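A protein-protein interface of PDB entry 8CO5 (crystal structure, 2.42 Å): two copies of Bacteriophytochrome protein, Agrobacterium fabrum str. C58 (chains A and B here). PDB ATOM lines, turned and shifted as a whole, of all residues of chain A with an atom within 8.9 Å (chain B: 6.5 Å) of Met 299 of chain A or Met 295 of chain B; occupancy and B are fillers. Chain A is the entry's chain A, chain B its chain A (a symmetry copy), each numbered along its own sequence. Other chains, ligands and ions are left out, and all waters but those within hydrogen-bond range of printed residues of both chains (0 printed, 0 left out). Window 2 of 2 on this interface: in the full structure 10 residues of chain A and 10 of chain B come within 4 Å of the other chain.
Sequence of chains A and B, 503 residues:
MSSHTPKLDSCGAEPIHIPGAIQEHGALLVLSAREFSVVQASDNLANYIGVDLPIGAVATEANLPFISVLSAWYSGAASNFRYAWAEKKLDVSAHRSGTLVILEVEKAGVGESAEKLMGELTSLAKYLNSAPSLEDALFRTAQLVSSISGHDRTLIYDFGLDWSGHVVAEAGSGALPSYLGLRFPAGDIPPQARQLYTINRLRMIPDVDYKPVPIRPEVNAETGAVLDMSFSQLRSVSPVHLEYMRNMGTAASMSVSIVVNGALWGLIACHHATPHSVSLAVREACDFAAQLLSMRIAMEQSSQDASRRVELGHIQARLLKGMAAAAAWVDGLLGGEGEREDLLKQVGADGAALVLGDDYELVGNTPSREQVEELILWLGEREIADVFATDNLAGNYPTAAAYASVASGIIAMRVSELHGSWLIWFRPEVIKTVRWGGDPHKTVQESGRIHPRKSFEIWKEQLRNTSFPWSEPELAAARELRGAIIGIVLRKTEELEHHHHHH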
ATOM      1  N   LEU A 124     -18.965 -36.843 -32.805  1.00  0.00           N
ATOM      2  CA  LEU A 124     -19.839 -36.373 -31.694  1.00  0.00           C
ATOM      3  C   LEU A 124     -19.040 -35.472 -30.744  1.00  0.00           C
ATOM      4  O   LEU A 124     -19.598 -34.453 -30.293  1.00  0.00           O
ATOM      5  CB  LEU A 124     -20.406 -37.590 -30.958  1.00  0.00           C
ATOM      6  CG  LEU A 124     -21.498 -37.288 -29.933  1.00  0.00           C
ATOM      7  CD1 LEU A 124     -22.714 -36.663 -30.599  1.00  0.00           C
ATOM      8  CD2 LEU A 124     -21.892 -38.549 -29.179  1.00  0.00           C
ATOM      9  N   ALA A 125     -17.791 -35.845 -30.443  1.00  0.00           N
ATOM     10  CA  ALA A 125     -16.864 -35.083 -29.573  1.00  0.00           C
ATOM     11  C   ALA A 125     -16.557 -33.724 -30.211  1.00  0.00           C
ATOM     12  O   ALA A 125     -16.442 -32.730 -29.464  1.00  0.00           O
ATOM     13  CB  ALA A 125     -15.604 -35.878 -29.337  1.00  0.00           C
ATOM     14  N   LYS A 126     -16.430 -33.691 -31.543  1.00  0.00           N
ATOM     15  CA  LYS A 126     -16.199 -32.455 -32.340  1.00  0.00           C
ATOM     16  C   LYS A 126     -17.491 -31.631 -32.378  1.00  0.00           C
ATOM     17  O   LYS A 126     -17.403 -30.390 -32.288  1.00  0.00           O
ATOM     18  CB  LYS A 126     -15.739 -32.810 -33.758  1.00  0.00           C
ATOM     19  N   LEU A 128     -20.040 -31.481 -30.176  1.00  0.00           N
ATOM     20  CA  LEU A 128     -20.528 -30.984 -28.859  1.00  0.00           C
ATOM     21  C   LEU A 128     -19.359 -30.512 -27.984  1.00  0.00           C
ATOM     22  O   LEU A 128     -19.370 -30.821 -26.776  1.00  0.00           O
ATOM     23  CB  LEU A 128     -21.314 -32.104 -28.171  1.00  0.00           C
ATOM     24  N   ASN A 129     -18.391 -29.799 -28.572  1.00  0.00           N
ATOM     25  CA  ASN A 129     -17.435 -28.927 -27.834  1.00  0.00           C
ATOM     26  C   ASN A 129     -17.592 -27.492 -28.355  1.00  0.00           C
ATOM     27  O   ASN A 129     -17.149 -26.558 -27.659  1.00  0.00           O
ATOM     28  CB  ASN A 129     -15.989 -29.423 -27.922  1.00  0.00           C
ATOM     29  CG  ASN A 129     -15.135 -28.932 -26.771  1.00  0.00           C
ATOM     30  OD1 ASN A 129     -15.588 -28.141 -25.946  1.00  0.00           O
ATOM     31  ND2 ASN A 129     -13.899 -29.397 -26.697  1.00  0.00           N
ATOM     32  N   SER A 130     -18.204 -27.339 -29.534  1.00  0.00           N
ATOM     33  CA  SER A 130     -18.765 -26.062 -30.049  1.00  0.00           C
ATOM     34  C   SER A 130     -19.845 -25.572 -29.077  1.00  0.00           C
ATOM     35  O   SER A 130     -20.173 -24.370 -29.107  1.00  0.00           O
ATOM     36  CB  SER A 130     -19.313 -26.230 -31.443  1.00  0.00           C
ATOM     37  N   ALA A 131     -20.371 -26.492 -28.259  1.00  0.00           N
ATOM     38  CA  ALA A 131     -21.293 -26.235 -27.125  1.00  0.00           C
ATOM     39  C   ALA A 131     -22.652 -25.770 -27.643  1.00  0.00           C
ATOM     40  O   ALA A 131     -23.110 -24.682 -27.299  1.00  0.00           O
ATOM     41  CB  ALA A 131     -20.677 -25.226 -26.186  1.00  0.00           C
ATOM     42  N   PRO A 132     -23.341 -26.580 -28.480  1.00  0.00           N
ATOM     43  CA  PRO A 132     -24.679 -26.237 -28.963  1.00  0.00           C
ATOM     44  C   PRO A 132     -25.791 -26.554 -27.949  1.00  0.00           C
ATOM     45  O   PRO A 132     -25.485 -26.774 -26.791  1.00  0.00           O
ATOM     46  CB  PRO A 132     -24.809 -27.133 -30.201  1.00  0.00           C
ATOM     47  CG  PRO A 132     -24.046 -28.379 -29.813  1.00  0.00           C
ATOM     48  CD  PRO A 132     -22.859 -27.860 -29.027  1.00  0.00           C
ATOM     49  N   VAL A 260     -23.335 -36.953 -13.755  1.00  0.00           N
ATOM     50  CA  VAL A 260     -22.977 -35.503 -13.798  1.00  0.00           C
ATOM     51  C   VAL A 260     -22.883 -34.978 -12.361  1.00  0.00           C
ATOM     52  O   VAL A 260     -23.866 -35.136 -11.610  1.00  0.00           O
ATOM     53  CB  VAL A 260     -24.001 -34.703 -14.630  1.00  0.00           C
ATOM     54  CG1 VAL A 260     -23.787 -33.203 -14.507  1.00  0.00           C
ATOM     55  CG2 VAL A 260     -23.992 -35.126 -16.091  1.00  0.00           C
ATOM     56  N   ASN A 261     -21.735 -34.392 -12.006  1.00  0.00           N
ATOM     57  CA  ASN A 261     -21.482 -33.779 -10.674  1.00  0.00           C
ATOM     58  C   ASN A 261     -21.672 -34.838  -9.579  1.00  0.00           C
ATOM     59  O   ASN A 261     -22.159 -34.475  -8.488  1.00  0.00           O
ATOM     60  CB  ASN A 261     -22.370 -32.551 -10.451  1.00  0.00           C
ATOM     61  CG  ASN A 261     -22.205 -31.501 -11.531  1.00  0.00           C
ATOM     62  OD1 ASN A 261     -21.205 -31.490 -12.246  1.00  0.00           O
ATOM     63  ND2 ASN A 261     -23.178 -30.615 -11.657  1.00  0.00           N
ATOM     64  N   GLN A 291     -19.948 -40.195 -21.172  1.00  0.00           N
ATOM     65  CA  GLN A 291     -19.040 -39.281 -20.427  1.00  0.00           C
ATOM     66  C   GLN A 291     -18.907 -37.960 -21.196  1.00  0.00           C
ATOM     67  O   GLN A 291     -18.892 -36.904 -20.537  1.00  0.00           O
ATOM     68  CB  GLN A 291     -17.686 -39.949 -20.172  1.00  0.00           C
ATOM     69  CG  GLN A 291     -17.673 -40.813 -18.917  1.00  0.00           C
ATOM     70  CD  GLN A 291     -16.360 -41.520 -18.681  1.00  0.00           C
ATOM     71  OE1 GLN A 291     -16.325 -42.711 -18.382  1.00  0.00           O
ATOM     72  NE2 GLN A 291     -15.263 -40.791 -18.805  1.00  0.00           N
ATOM     73  N   LEU A 292     -18.831 -38.015 -22.532  1.00  0.00           N
ATOM     74  CA  LEU A 292     -18.793 -36.815 -23.413  1.00  0.00           C
ATOM     75  C   LEU A 292     -20.067 -35.992 -23.189  1.00  0.00           C
ATOM     76  O   LEU A 292     -19.949 -34.779 -22.926  1.00  0.00           O
ATOM     77  CB  LEU A 292     -18.670 -37.242 -24.880  1.00  0.00           C
ATOM     78  CG  LEU A 292     -17.350 -37.901 -25.278  1.00  0.00           C
ATOM     79  CD1 LEU A 292     -17.362 -38.279 -26.751  1.00  0.00           C
ATOM     80  CD2 LEU A 292     -16.166 -36.996 -24.972  1.00  0.00           C
ATOM     81  N   LEU A 293     -21.233 -36.638 -23.295  1.00  0.00           N
ATOM     82  CA  LEU A 293     -22.564 -36.029 -23.022  1.00  0.00           C
ATOM     83  C   LEU A 293     -22.569 -35.464 -21.597  1.00  0.00           C
ATOM     84  O   LEU A 293     -23.002 -34.310 -21.420  1.00  0.00           O
ATOM     85  CB  LEU A 293     -23.654 -37.089 -23.207  1.00  0.00           C
ATOM     86  CG  LEU A 293     -25.063 -36.675 -22.781  1.00  0.00           C
ATOM     87  CD1 LEU A 293     -25.481 -35.372 -23.447  1.00  0.00           C
ATOM     88  CD2 LEU A 293     -26.069 -37.775 -23.090  1.00  0.00           C
ATOM     89  N   SER A 294     -22.092 -36.256 -20.630  1.00  0.00           N
ATOM     90  CA  SER A 294     -22.002 -35.901 -19.189  1.00  0.00           C
ATOM     91  C   SER A 294     -21.175 -34.621 -19.011  1.00  0.00           C
ATOM     92  O   SER A 294     -21.639 -33.721 -18.284  1.00  0.00           O
ATOM     93  CB  SER A 294     -21.428 -37.042 -18.385  1.00  0.00           C
ATOM     94  OG  SER A 294     -21.143 -36.636 -17.054  1.00  0.00           O
ATOM     95  N   MET A 295     -20.005 -34.548 -19.656  1.00  0.00           N
ATOM     96  CA  MET A 295     -19.081 -33.381 -19.584  1.00  0.00           C
ATOM     97  C   MET A 295     -19.826 -32.118 -20.034  1.00  0.00           C
ATOM     98  O   MET A 295     -19.564 -31.041 -19.460  1.00  0.00           O
ATOM     99  CB  MET A 295     -17.847 -33.575 -20.472  1.00  0.00           C
ATOM    100  CG  MET A 295     -17.008 -34.787 -20.106  1.00  0.00           C
ATOM    101  SD  MET A 295     -15.230 -34.520 -20.344  1.00  0.00           S
ATOM    102  CE  MET A 295     -14.839 -33.586 -18.866  1.00  0.00           C
ATOM    103  N   ARG A 296     -20.721 -32.254 -21.018  1.00  0.00           N
ATOM    104  CA  ARG A 296     -21.450 -31.127 -21.661  1.00  0.00           C
ATOM    105  C   ARG A 296     -22.620 -30.682 -20.777  1.00  0.00           C
ATOM    106  O   ARG A 296     -22.762 -29.461 -20.568  1.00  0.00           O
ATOM    107  CB  ARG A 296     -21.934 -31.525 -23.058  1.00  0.00           C
ATOM    108  CG  ARG A 296     -21.063 -30.993 -24.187  1.00  0.00           C
ATOM    109  CD  ARG A 296     -21.083 -29.476 -24.250  1.00  0.00           C
ATOM    110  NE  ARG A 296     -22.428 -28.957 -24.463  1.00  0.00           N
ATOM    111  CZ  ARG A 296     -22.816 -27.712 -24.200  1.00  0.00           C
ATOM    112  NH1 ARG A 296     -21.961 -26.836 -23.699  1.00  0.00           N
ATOM    113  NH2 ARG A 296     -24.064 -27.348 -24.436  1.00  0.00           N
ATOM    114  N   ILE A 297     -23.431 -31.631 -20.295  1.00  0.00           N
ATOM    115  CA  ILE A 297     -24.612 -31.360 -19.419  1.00  0.00           C
ATOM    116  C   ILE A 297     -24.154 -30.483 -18.246  1.00  0.00           C
ATOM    117  O   ILE A 297     -24.844 -29.489 -17.946  1.00  0.00           O
ATOM    118  CB  ILE A 297     -25.267 -32.671 -18.937  1.00  0.00           C
ATOM    119  CG1 ILE A 297     -25.894 -33.448 -20.098  1.00  0.00           C
ATOM    120  CG2 ILE A 297     -26.280 -32.397 -17.834  1.00  0.00           C
ATOM    121  CD1 ILE A 297     -26.500 -34.775 -19.701  1.00  0.00           C
ATOM    122  N   ALA A 298     -23.026 -30.843 -17.626  1.00  0.00           N
ATOM    123  CA  ALA A 298     -22.419 -30.146 -16.467  1.00  0.00           C
ATOM    124  C   ALA A 298     -22.131 -28.681 -16.820  1.00  0.00           C
ATOM    125  O   ALA A 298     -22.452 -27.802 -15.996  1.00  0.00           O
ATOM    126  CB  ALA A 298     -21.158 -30.859 -16.045  1.00  0.00           C
ATOM    127  N   MET A 299     -21.557 -28.440 -18.004  1.00  0.00           N
ATOM    128  CA  MET A 299     -21.094 -27.098 -18.456  1.00  0.00           C
ATOM    129  C   MET A 299     -22.301 -26.196 -18.744  1.00  0.00           C
ATOM    130  O   MET A 299     -22.288 -25.038 -18.282  1.00  0.00           O
ATOM    131  CB  MET A 299     -20.230 -27.210 -19.716  1.00  0.00           C
ATOM    132  CG  MET A 299     -18.753 -27.387 -19.421  1.00  0.00           C
ATOM    133  SD  MET A 299     -17.870 -28.271 -20.733  1.00  0.00           S
ATOM    134  CE  MET A 299     -18.441 -27.379 -22.178  1.00  0.00           C
ATOM    135  N   GLU A 300     -23.290 -26.709 -19.485  1.00  0.00           N
ATOM    136  CA  GLU A 300     -24.503 -25.935 -19.870  1.00  0.00           C
ATOM    137  C   GLU A 300     -25.298 -25.591 -18.605  1.00  0.00           C
ATOM    138  O   GLU A 300     -25.738 -24.430 -18.487  1.00  0.00           O
ATOM    139  CB  GLU A 300     -25.366 -26.698 -20.876  1.00  0.00           C
ATOM    140  CG  GLU A 300     -26.428 -25.824 -21.527  1.00  0.00           C
ATOM    141  CD  GLU A 300     -27.177 -26.461 -22.686  1.00  0.00           C
ATOM    142  OE1 GLU A 300     -26.835 -27.603 -23.055  1.00  0.00           O
ATOM    143  OE2 GLU A 300     -28.098 -25.810 -23.219  1.00  0.00           O
ATOM    144  N   GLN A 301     -25.470 -26.561 -17.701  1.00  0.00           N
ATOM    145  CA  GLN A 301     -26.085 -26.360 -16.360  1.00  0.00           C
ATOM    146  C   GLN A 301     -25.315 -25.266 -15.614  1.00  0.00           C
ATOM    147  O   GLN A 301     -25.963 -24.352 -15.068  1.00  0.00           O
ATOM    148  CB  GLN A 301     -26.065 -27.658 -15.547  1.00  0.00           C
ATOM    149  CG  GLN A 301     -27.157 -28.644 -15.934  1.00  0.00           C
ATOM    150  CD  GLN A 301     -27.179 -29.848 -15.025  1.00  0.00           C
ATOM    151  OE1 GLN A 301     -26.278 -30.059 -14.216  1.00  0.00           O
ATOM    152  NE2 GLN A 301     -28.219 -30.656 -15.153  1.00  0.00           N
ATOM    153  N   SER A 302     -23.983 -25.370 -15.600  1.00  0.00           N
ATOM    154  CA  SER A 302     -23.048 -24.450 -14.900  1.00  0.00           C
ATOM    155  C   SER A 302     -23.175 -23.033 -15.469  1.00  0.00           C
ATOM    156  O   SER A 302     -23.188 -22.075 -14.671  1.00  0.00           O
ATOM    157  CB  SER A 302     -21.628 -24.952 -14.991  1.00  0.00           C
ATOM    158  OG  SER A 302     -20.756 -24.167 -14.193  1.00  0.00           O
ATOM    159  N   SER A 303     -23.270 -22.913 -16.799  1.00  0.00           N
ATOM    160  CA  SER A 303     -23.292 -21.625 -17.544  1.00  0.00           C
ATOM    161  C   SER A 303     -24.690 -20.996 -17.483  1.00  0.00           C
ATOM    162  O   SER A 303     -24.771 -19.768 -17.283  1.00  0.00           O
ATOM    163  CB  SER A 303     -22.833 -21.814 -18.968  1.00  0.00           C
ATOM    164  OG  SER A 303     -23.772 -22.580 -19.709  1.00  0.00           O
ATOM    165  N   GLN A 304     -25.742 -21.802 -17.664  1.00  0.00           N
ATOM    166  CA  GLN A 304     -27.162 -21.354 -17.588  1.00  0.00           C
ATOM    167  C   GLN A 304     -27.450 -20.827 -16.176  1.00  0.00           C
ATOM    168  O   GLN A 304     -28.137 -19.793 -16.061  1.00  0.00           O
ATOM    169  CB  GLN A 304     -28.121 -22.489 -17.950  1.00  0.00           C
ATOM    170  CG  GLN A 304     -28.265 -22.714 -19.449  1.00  0.00           C
ATOM    171  CD  GLN A 304     -29.285 -23.776 -19.777  1.00  0.00           C
ATOM    172  OE1 GLN A 304     -30.034 -24.233 -18.917  1.00  0.00           O
ATOM    173  NE2 GLN A 304     -29.322 -24.180 -21.037  1.00  0.00           N
ATOM    174  N   ASP A 305     -26.942 -21.520 -15.151  1.00  0.00           N
ATOM    175  CA  ASP A 305     -27.079 -21.133 -13.720  1.00  0.00           C
ATOM    176  C   ASP A 305     -26.331 -19.815 -13.488  1.00  0.00           C
ATOM    177  O   ASP A 305     -26.884 -18.938 -12.797  1.00  0.00           O
ATOM    178  CB  ASP A 305     -26.570 -22.241 -12.794  1.00  0.00           C
ATOM    179  CG  ASP A 305     -26.763 -21.945 -11.316  1.00  0.00           C
ATOM    180  OD1 ASP A 305     -26.018 -21.098 -10.786  1.00  0.00           O
ATOM    181  OD2 ASP A 305     -27.662 -22.561 -10.708  1.00  0.00           O
ATOM    182  N   ALA A 306     -25.124 -19.692 -14.050  1.00  0.00           N
ATOM    183  CA  ALA A 306     -24.251 -18.496 -13.953  1.00  0.00           C
ATOM    184  C   ALA A 306     -24.957 -17.290 -14.583  1.00  0.00           C
ATOM    185  O   ALA A 306     -25.015 -16.230 -13.930  1.00  0.00           O
ATOM    186  CB  ALA A 306     -22.924 -18.769 -14.617  1.00  0.00           C
ATOM    187  N   SER A 307     -25.474 -17.458 -15.804  1.00  0.00           N
ATOM    188  CA  SER A 307     -26.186 -16.415 -16.592  1.00  0.00           C
ATOM    189  C   SER A 307     -27.421 -15.927 -15.826  1.00  0.00           C
ATOM    190  O   SER A 307     -27.699 -14.710 -15.865  1.00  0.00           O
ATOM    191  CB  SER A 307     -26.562 -16.933 -17.957  1.00  0.00           C
ATOM    192  OG  SER A 307     -25.405 -17.274 -18.706  1.00  0.00           O
ATOM    193  N   VAL B 259      -8.078 -24.460 -26.429  1.00  0.00           N
ATOM    194  CA  VAL B 259      -9.082 -23.358 -26.493  1.00  0.00           C
ATOM    195  C   VAL B 259     -10.143 -23.604 -25.416  1.00  0.00           C
ATOM    196  O   VAL B 259     -10.864 -24.616 -25.512  1.00  0.00           O
ATOM    197  CB  VAL B 259      -9.710 -23.248 -27.897  1.00  0.00           C
ATOM    198  CG1 VAL B 259     -10.786 -22.174 -27.955  1.00  0.00           C
ATOM    199  CG2 VAL B 259      -8.652 -23.000 -28.961  1.00  0.00           C
ATOM    200  N   VAL B 260     -10.222 -22.705 -24.431  1.00  0.00           N
ATOM    201  CA  VAL B 260     -11.164 -22.782 -23.275  1.00  0.00           C
ATOM    202  C   VAL B 260     -12.024 -21.513 -23.258  1.00  0.00           C
ATOM    203  O   VAL B 260     -11.446 -20.410 -23.243  1.00  0.00           O
ATOM    204  CB  VAL B 260     -10.402 -22.970 -21.948  1.00  0.00           C
ATOM    205  CG1 VAL B 260     -11.317 -22.830 -20.740  1.00  0.00           C
ATOM    206  CG2 VAL B 260      -9.663 -24.299 -21.907  1.00  0.00           C
ATOM    207  N   ALA B 290      -6.225 -32.429 -26.477  1.00  0.00           N
ATOM    208  CA  ALA B 290      -6.208 -30.976 -26.181  1.00  0.00           C
ATOM    209  C   ALA B 290      -7.622 -30.507 -25.817  1.00  0.00           C
ATOM    210  O   ALA B 290      -7.744 -29.608 -24.963  1.00  0.00           O
ATOM    211  CB  ALA B 290      -5.666 -30.212 -27.363  1.00  0.00           C
ATOM    212  N   GLN B 291      -8.643 -31.099 -26.444  1.00  0.00           N
ATOM    213  CA  GLN B 291     -10.077 -30.784 -26.193  1.00  0.00           C
ATOM    214  C   GLN B 291     -10.507 -31.408 -24.858  1.00  0.00           C
ATOM    215  O   GLN B 291     -11.257 -30.742 -24.121  1.00  0.00           O
ATOM    216  CB  GLN B 291     -10.948 -31.247 -27.363  1.00  0.00           C
ATOM    217  CG  GLN B 291     -11.030 -30.221 -28.487  1.00  0.00           C
ATOM    218  CD  GLN B 291     -11.843 -30.684 -29.672  1.00  0.00           C
ATOM    219  OE1 GLN B 291     -11.431 -30.542 -30.822  1.00  0.00           O
ATOM    220  NE2 GLN B 291     -13.015 -31.239 -29.407  1.00  0.00           N
ATOM    221  N   LEU B 292     -10.039 -32.625 -24.554  1.00  0.00           N
ATOM    222  CA  LEU B 292     -10.296 -33.314 -23.259  1.00  0.00           C
ATOM    223  C   LEU B 292      -9.741 -32.453 -22.118  1.00  0.00           C
ATOM    224  O   LEU B 292     -10.497 -32.171 -21.169  1.00  0.00           O
ATOM    225  CB  LEU B 292      -9.645 -34.702 -23.263  1.00  0.00           C
ATOM    226  CG  LEU B 292     -10.248 -35.723 -24.226  1.00  0.00           C
ATOM    227  CD1 LEU B 292      -9.508 -37.050 -24.135  1.00  0.00           C
ATOM    228  CD2 LEU B 292     -11.733 -35.924 -23.960  1.00  0.00           C
ATOM    229  N   LEU B 293      -8.465 -32.062 -22.218  1.00  0.00           N
ATOM    230  CA  LEU B 293      -7.783 -31.150 -21.259  1.00  0.00           C
ATOM    231  C   LEU B 293      -8.577 -29.842 -21.166  1.00  0.00           C
ATOM    232  O   LEU B 293      -8.832 -29.385 -20.037  1.00  0.00           O
ATOM    233  CB  LEU B 293      -6.347 -30.900 -21.731  1.00  0.00           C
ATOM    234  CG  LEU B 293      -5.569 -29.835 -20.958  1.00  0.00           C
ATOM    235  CD1 LEU B 293      -5.588 -30.115 -19.462  1.00  0.00           C
ATOM    236  CD2 LEU B 293      -4.136 -29.737 -21.461  1.00  0.00           C
ATOM    237  N   SER B 294      -8.956 -29.280 -22.319  1.00  0.00           N
ATOM    238  CA  SER B 294      -9.736 -28.022 -22.453  1.00  0.00           C
ATOM    239  C   SER B 294     -11.058 -28.137 -21.687  1.00  0.00           C
ATOM    240  O   SER B 294     -11.378 -27.202 -20.927  1.00  0.00           O
ATOM    241  CB  SER B 294      -9.967 -27.679 -23.904  1.00  0.00           C
ATOM    242  OG  SER B 294     -10.885 -26.603 -24.034  1.00  0.00           O
ATOM    243  N   MET B 295     -11.789 -29.242 -21.877  1.00  0.00           N
ATOM    244  CA  MET B 295     -13.099 -29.504 -21.216  1.00  0.00           C
ATOM    245  C   MET B 295     -12.919 -29.445 -19.694  1.00  0.00           C
ATOM    246  O   MET B 295     -13.844 -28.967 -19.008  1.00  0.00           O
ATOM    247  CB  MET B 295     -13.664 -30.877 -21.599  1.00  0.00           C
ATOM    248  CG  MET B 295     -13.913 -31.051 -23.087  1.00  0.00           C
ATOM    249  SD  MET B 295     -15.372 -32.061 -23.453  1.00  0.00           S
ATOM    250  CE  MET B 295     -16.676 -30.859 -23.198  1.00  0.00           C
ATOM    251  N   ARG B 296     -11.766 -29.909 -19.198  1.00  0.00           N
ATOM    252  CA  ARG B 296     -11.463 -30.038 -17.746  1.00  0.00           C
ATOM    253  C   ARG B 296     -11.063 -28.677 -17.166  1.00  0.00           C
ATOM    254  O   ARG B 296     -11.595 -28.320 -16.096  1.00  0.00           O
ATOM    255  CB  ARG B 296     -10.365 -31.081 -17.516  1.00  0.00           C
ATOM    256  CG  ARG B 296     -10.887 -32.434 -17.052  1.00  0.00           C
ATOM    257  CD  ARG B 296     -11.551 -32.346 -15.689  1.00  0.00           C
ATOM    258  NE  ARG B 296     -10.632 -31.864 -14.665  1.00  0.00           N
ATOM    259  CZ  ARG B 296     -10.998 -31.343 -13.496  1.00  0.00           C
ATOM    260  NH1 ARG B 296     -12.279 -31.222 -13.189  1.00  0.00           N
ATOM    261  NH2 ARG B 296     -10.077 -30.940 -12.639  1.00  0.00           N
ATOM    262  N   ILE B 297     -10.155 -27.960 -17.835  1.00  0.00           N
ATOM    263  CA  ILE B 297      -9.663 -26.615 -17.402  1.00  0.00           C
ATOM    264  C   ILE B 297     -10.878 -25.718 -17.137  1.00  0.00           C
ATOM    265  O   ILE B 297     -10.898 -25.045 -16.087  1.00  0.00           O
ATOM    266  CB  ILE B 297      -8.710 -26.001 -18.450  1.00  0.00           C
ATOM    267  CG1 ILE B 297      -7.410 -26.801 -18.567  1.00  0.00           C
ATOM    268  CG2 ILE B 297      -8.441 -24.535 -18.142  1.00  0.00           C
ATOM    269  CD1 ILE B 297      -6.457 -26.287 -19.622  1.00  0.00           C
ATOM    270  N   ALA B 298     -11.850 -25.726 -18.055  1.00  0.00           N
ATOM    271  CA  ALA B 298     -13.095 -24.926 -18.001  1.00  0.00           C
ATOM    272  C   ALA B 298     -13.874 -25.241 -16.716  1.00  0.00           C
ATOM    273  O   ALA B 298     -14.333 -24.289 -16.057  1.00  0.00           O
ATOM    274  CB  ALA B 298     -13.934 -25.200 -19.224  1.00  0.00           C
ATOM    275  N   MET B 299     -14.000 -26.530 -16.382  1.00  0.00           N
ATOM    276  CA  MET B 299     -14.825 -27.026 -15.243  1.00  0.00           C
ATOM    277  C   MET B 299     -14.166 -26.641 -13.913  1.00  0.00           C
ATOM    278  O   MET B 299     -14.888 -26.137 -13.028  1.00  0.00           O
ATOM    279  CB  MET B 299     -14.991 -28.547 -15.308  1.00  0.00           C
ATOM    280  CG  MET B 299     -16.205 -28.989 -16.104  1.00  0.00           C
ATOM    281  SD  MET B 299     -16.008 -30.633 -16.841  1.00  0.00           S
ATOM    282  CE  MET B 299     -15.422 -31.562 -15.426  1.00  0.00           C
ATOM    283  N   GLU B 300     -12.856 -26.879 -13.781  1.00  0.00           N
ATOM    284  CA  GLU B 300     -12.098 -26.587 -12.533  1.00  0.00           C
ATOM    285  C   GLU B 300     -12.096 -25.073 -12.291  1.00  0.00           C
ATOM    286  O   GLU B 300     -12.326 -24.664 -11.138  1.00  0.00           O
ATOM    287  CB  GLU B 300     -10.674 -27.141 -12.592  1.00  0.00           C
ATOM    288  CG  GLU B 300      -9.982 -27.146 -11.238  1.00  0.00           C
ATOM    289  CD  GLU B 300      -8.651 -27.875 -11.186  1.00  0.00           C
ATOM    290  OE1 GLU B 300      -8.256 -28.461 -12.216  1.00  0.00           O
ATOM    291  OE2 GLU B 300      -8.013 -27.861 -10.114  1.00  0.00           O
ATOM    292  N   SER B 302     -14.383 -23.017 -13.451  1.00  0.00           N
ATOM    293  CA  SER B 302     -15.823 -22.753 -13.191  1.00  0.00           C
ATOM    294  C   SER B 302     -16.164 -23.071 -11.731  1.00  0.00           C
ATOM    295  O   SER B 302     -16.899 -22.278 -11.110  1.00  0.00           O
ATOM    296  CB  SER B 302     -16.694 -23.535 -14.142  1.00  0.00           C
ATOM    297  OG  SER B 302     -18.058 -23.168 -14.006  1.00  0.00           O
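Among the printed residues, merely in contact across the chains: Ala 125 of chain A with Gln 291 of chain B, Asn 129 of chain A with Met 295 of chain B, Met 295 of chain A with Met 295 of chain B, Met 295 of chain A with Met 299 of chain B and Met 299 of chain A with Met 295 of chain B.
Of the 14 printed residues of chain B, 4 touch a printed residue of chain A.
Of the 27 printed residues of chain A, 5 touch a printed residue of chain B.
Along chain A the printed residues that touch a printed residue of chain B span positions 125 to 302.
Among the printed residues, 7 pairs touch across the chains.
Among the printed residues, no Asp or Glu carboxylate lies within 4 Å of a Lys or Arg side-chain nitrogen of the other chain.
Met 295 of chain A touches its own counterpart, Met 295 of chain B.
Met 295 of chain A touches Met 299 of chain B, and with the chains exchanged Met 299 of chain A touches Met 295 of chain B.
Ser 302 of chain B touches its own counterpart, Ser 302 of chain A.
Positions printed for both chains: 260, 291, 292, 293, 294, 295, 296, 297, 298, 299, 300 and 302.
Printed residues of chain B within 4 Å of Ala 125 of chain A: Gln 291 (3.7 Å).
Of the printed residues of chain B, Met 295 of chain A touches Met 295 and Met 299.
Of the printed residues of chain B, Met 299 of chain A touches Met 295.
Val 260 of chain B touches none of the printed residues of chain A.
Ala 290 of chain B touches none of the printed residues of chain A.
Of the printed residues of chain A, Gln 291 of chain B touches Ala 125 (3.7 Å) and Asn 129 (3.4 Å).
No residue of chain A comes within 4 Å of Ser 294 of chain B.
Of the printed residues of chain A, Met 295 of chain B touches Asn 129, Met 295 and Met 299.
The side-chain amide nitrogen (ND2) of Asn 129 of chain A sits close to the side-chain amide nitrogen (NE2) of Gln 291 of chain B, 3.4 Å away.
The side-chain hydroxyl of Ser 302 of chain A sits at hydrogen-bond distance from the side-chain hydroxyl of Ser 302 of chain B (2.9 Å).
O of Met 299 of chain A lies within hydrogen-bond range of OG of Ser 303 of chain A, at 3.2 Å.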
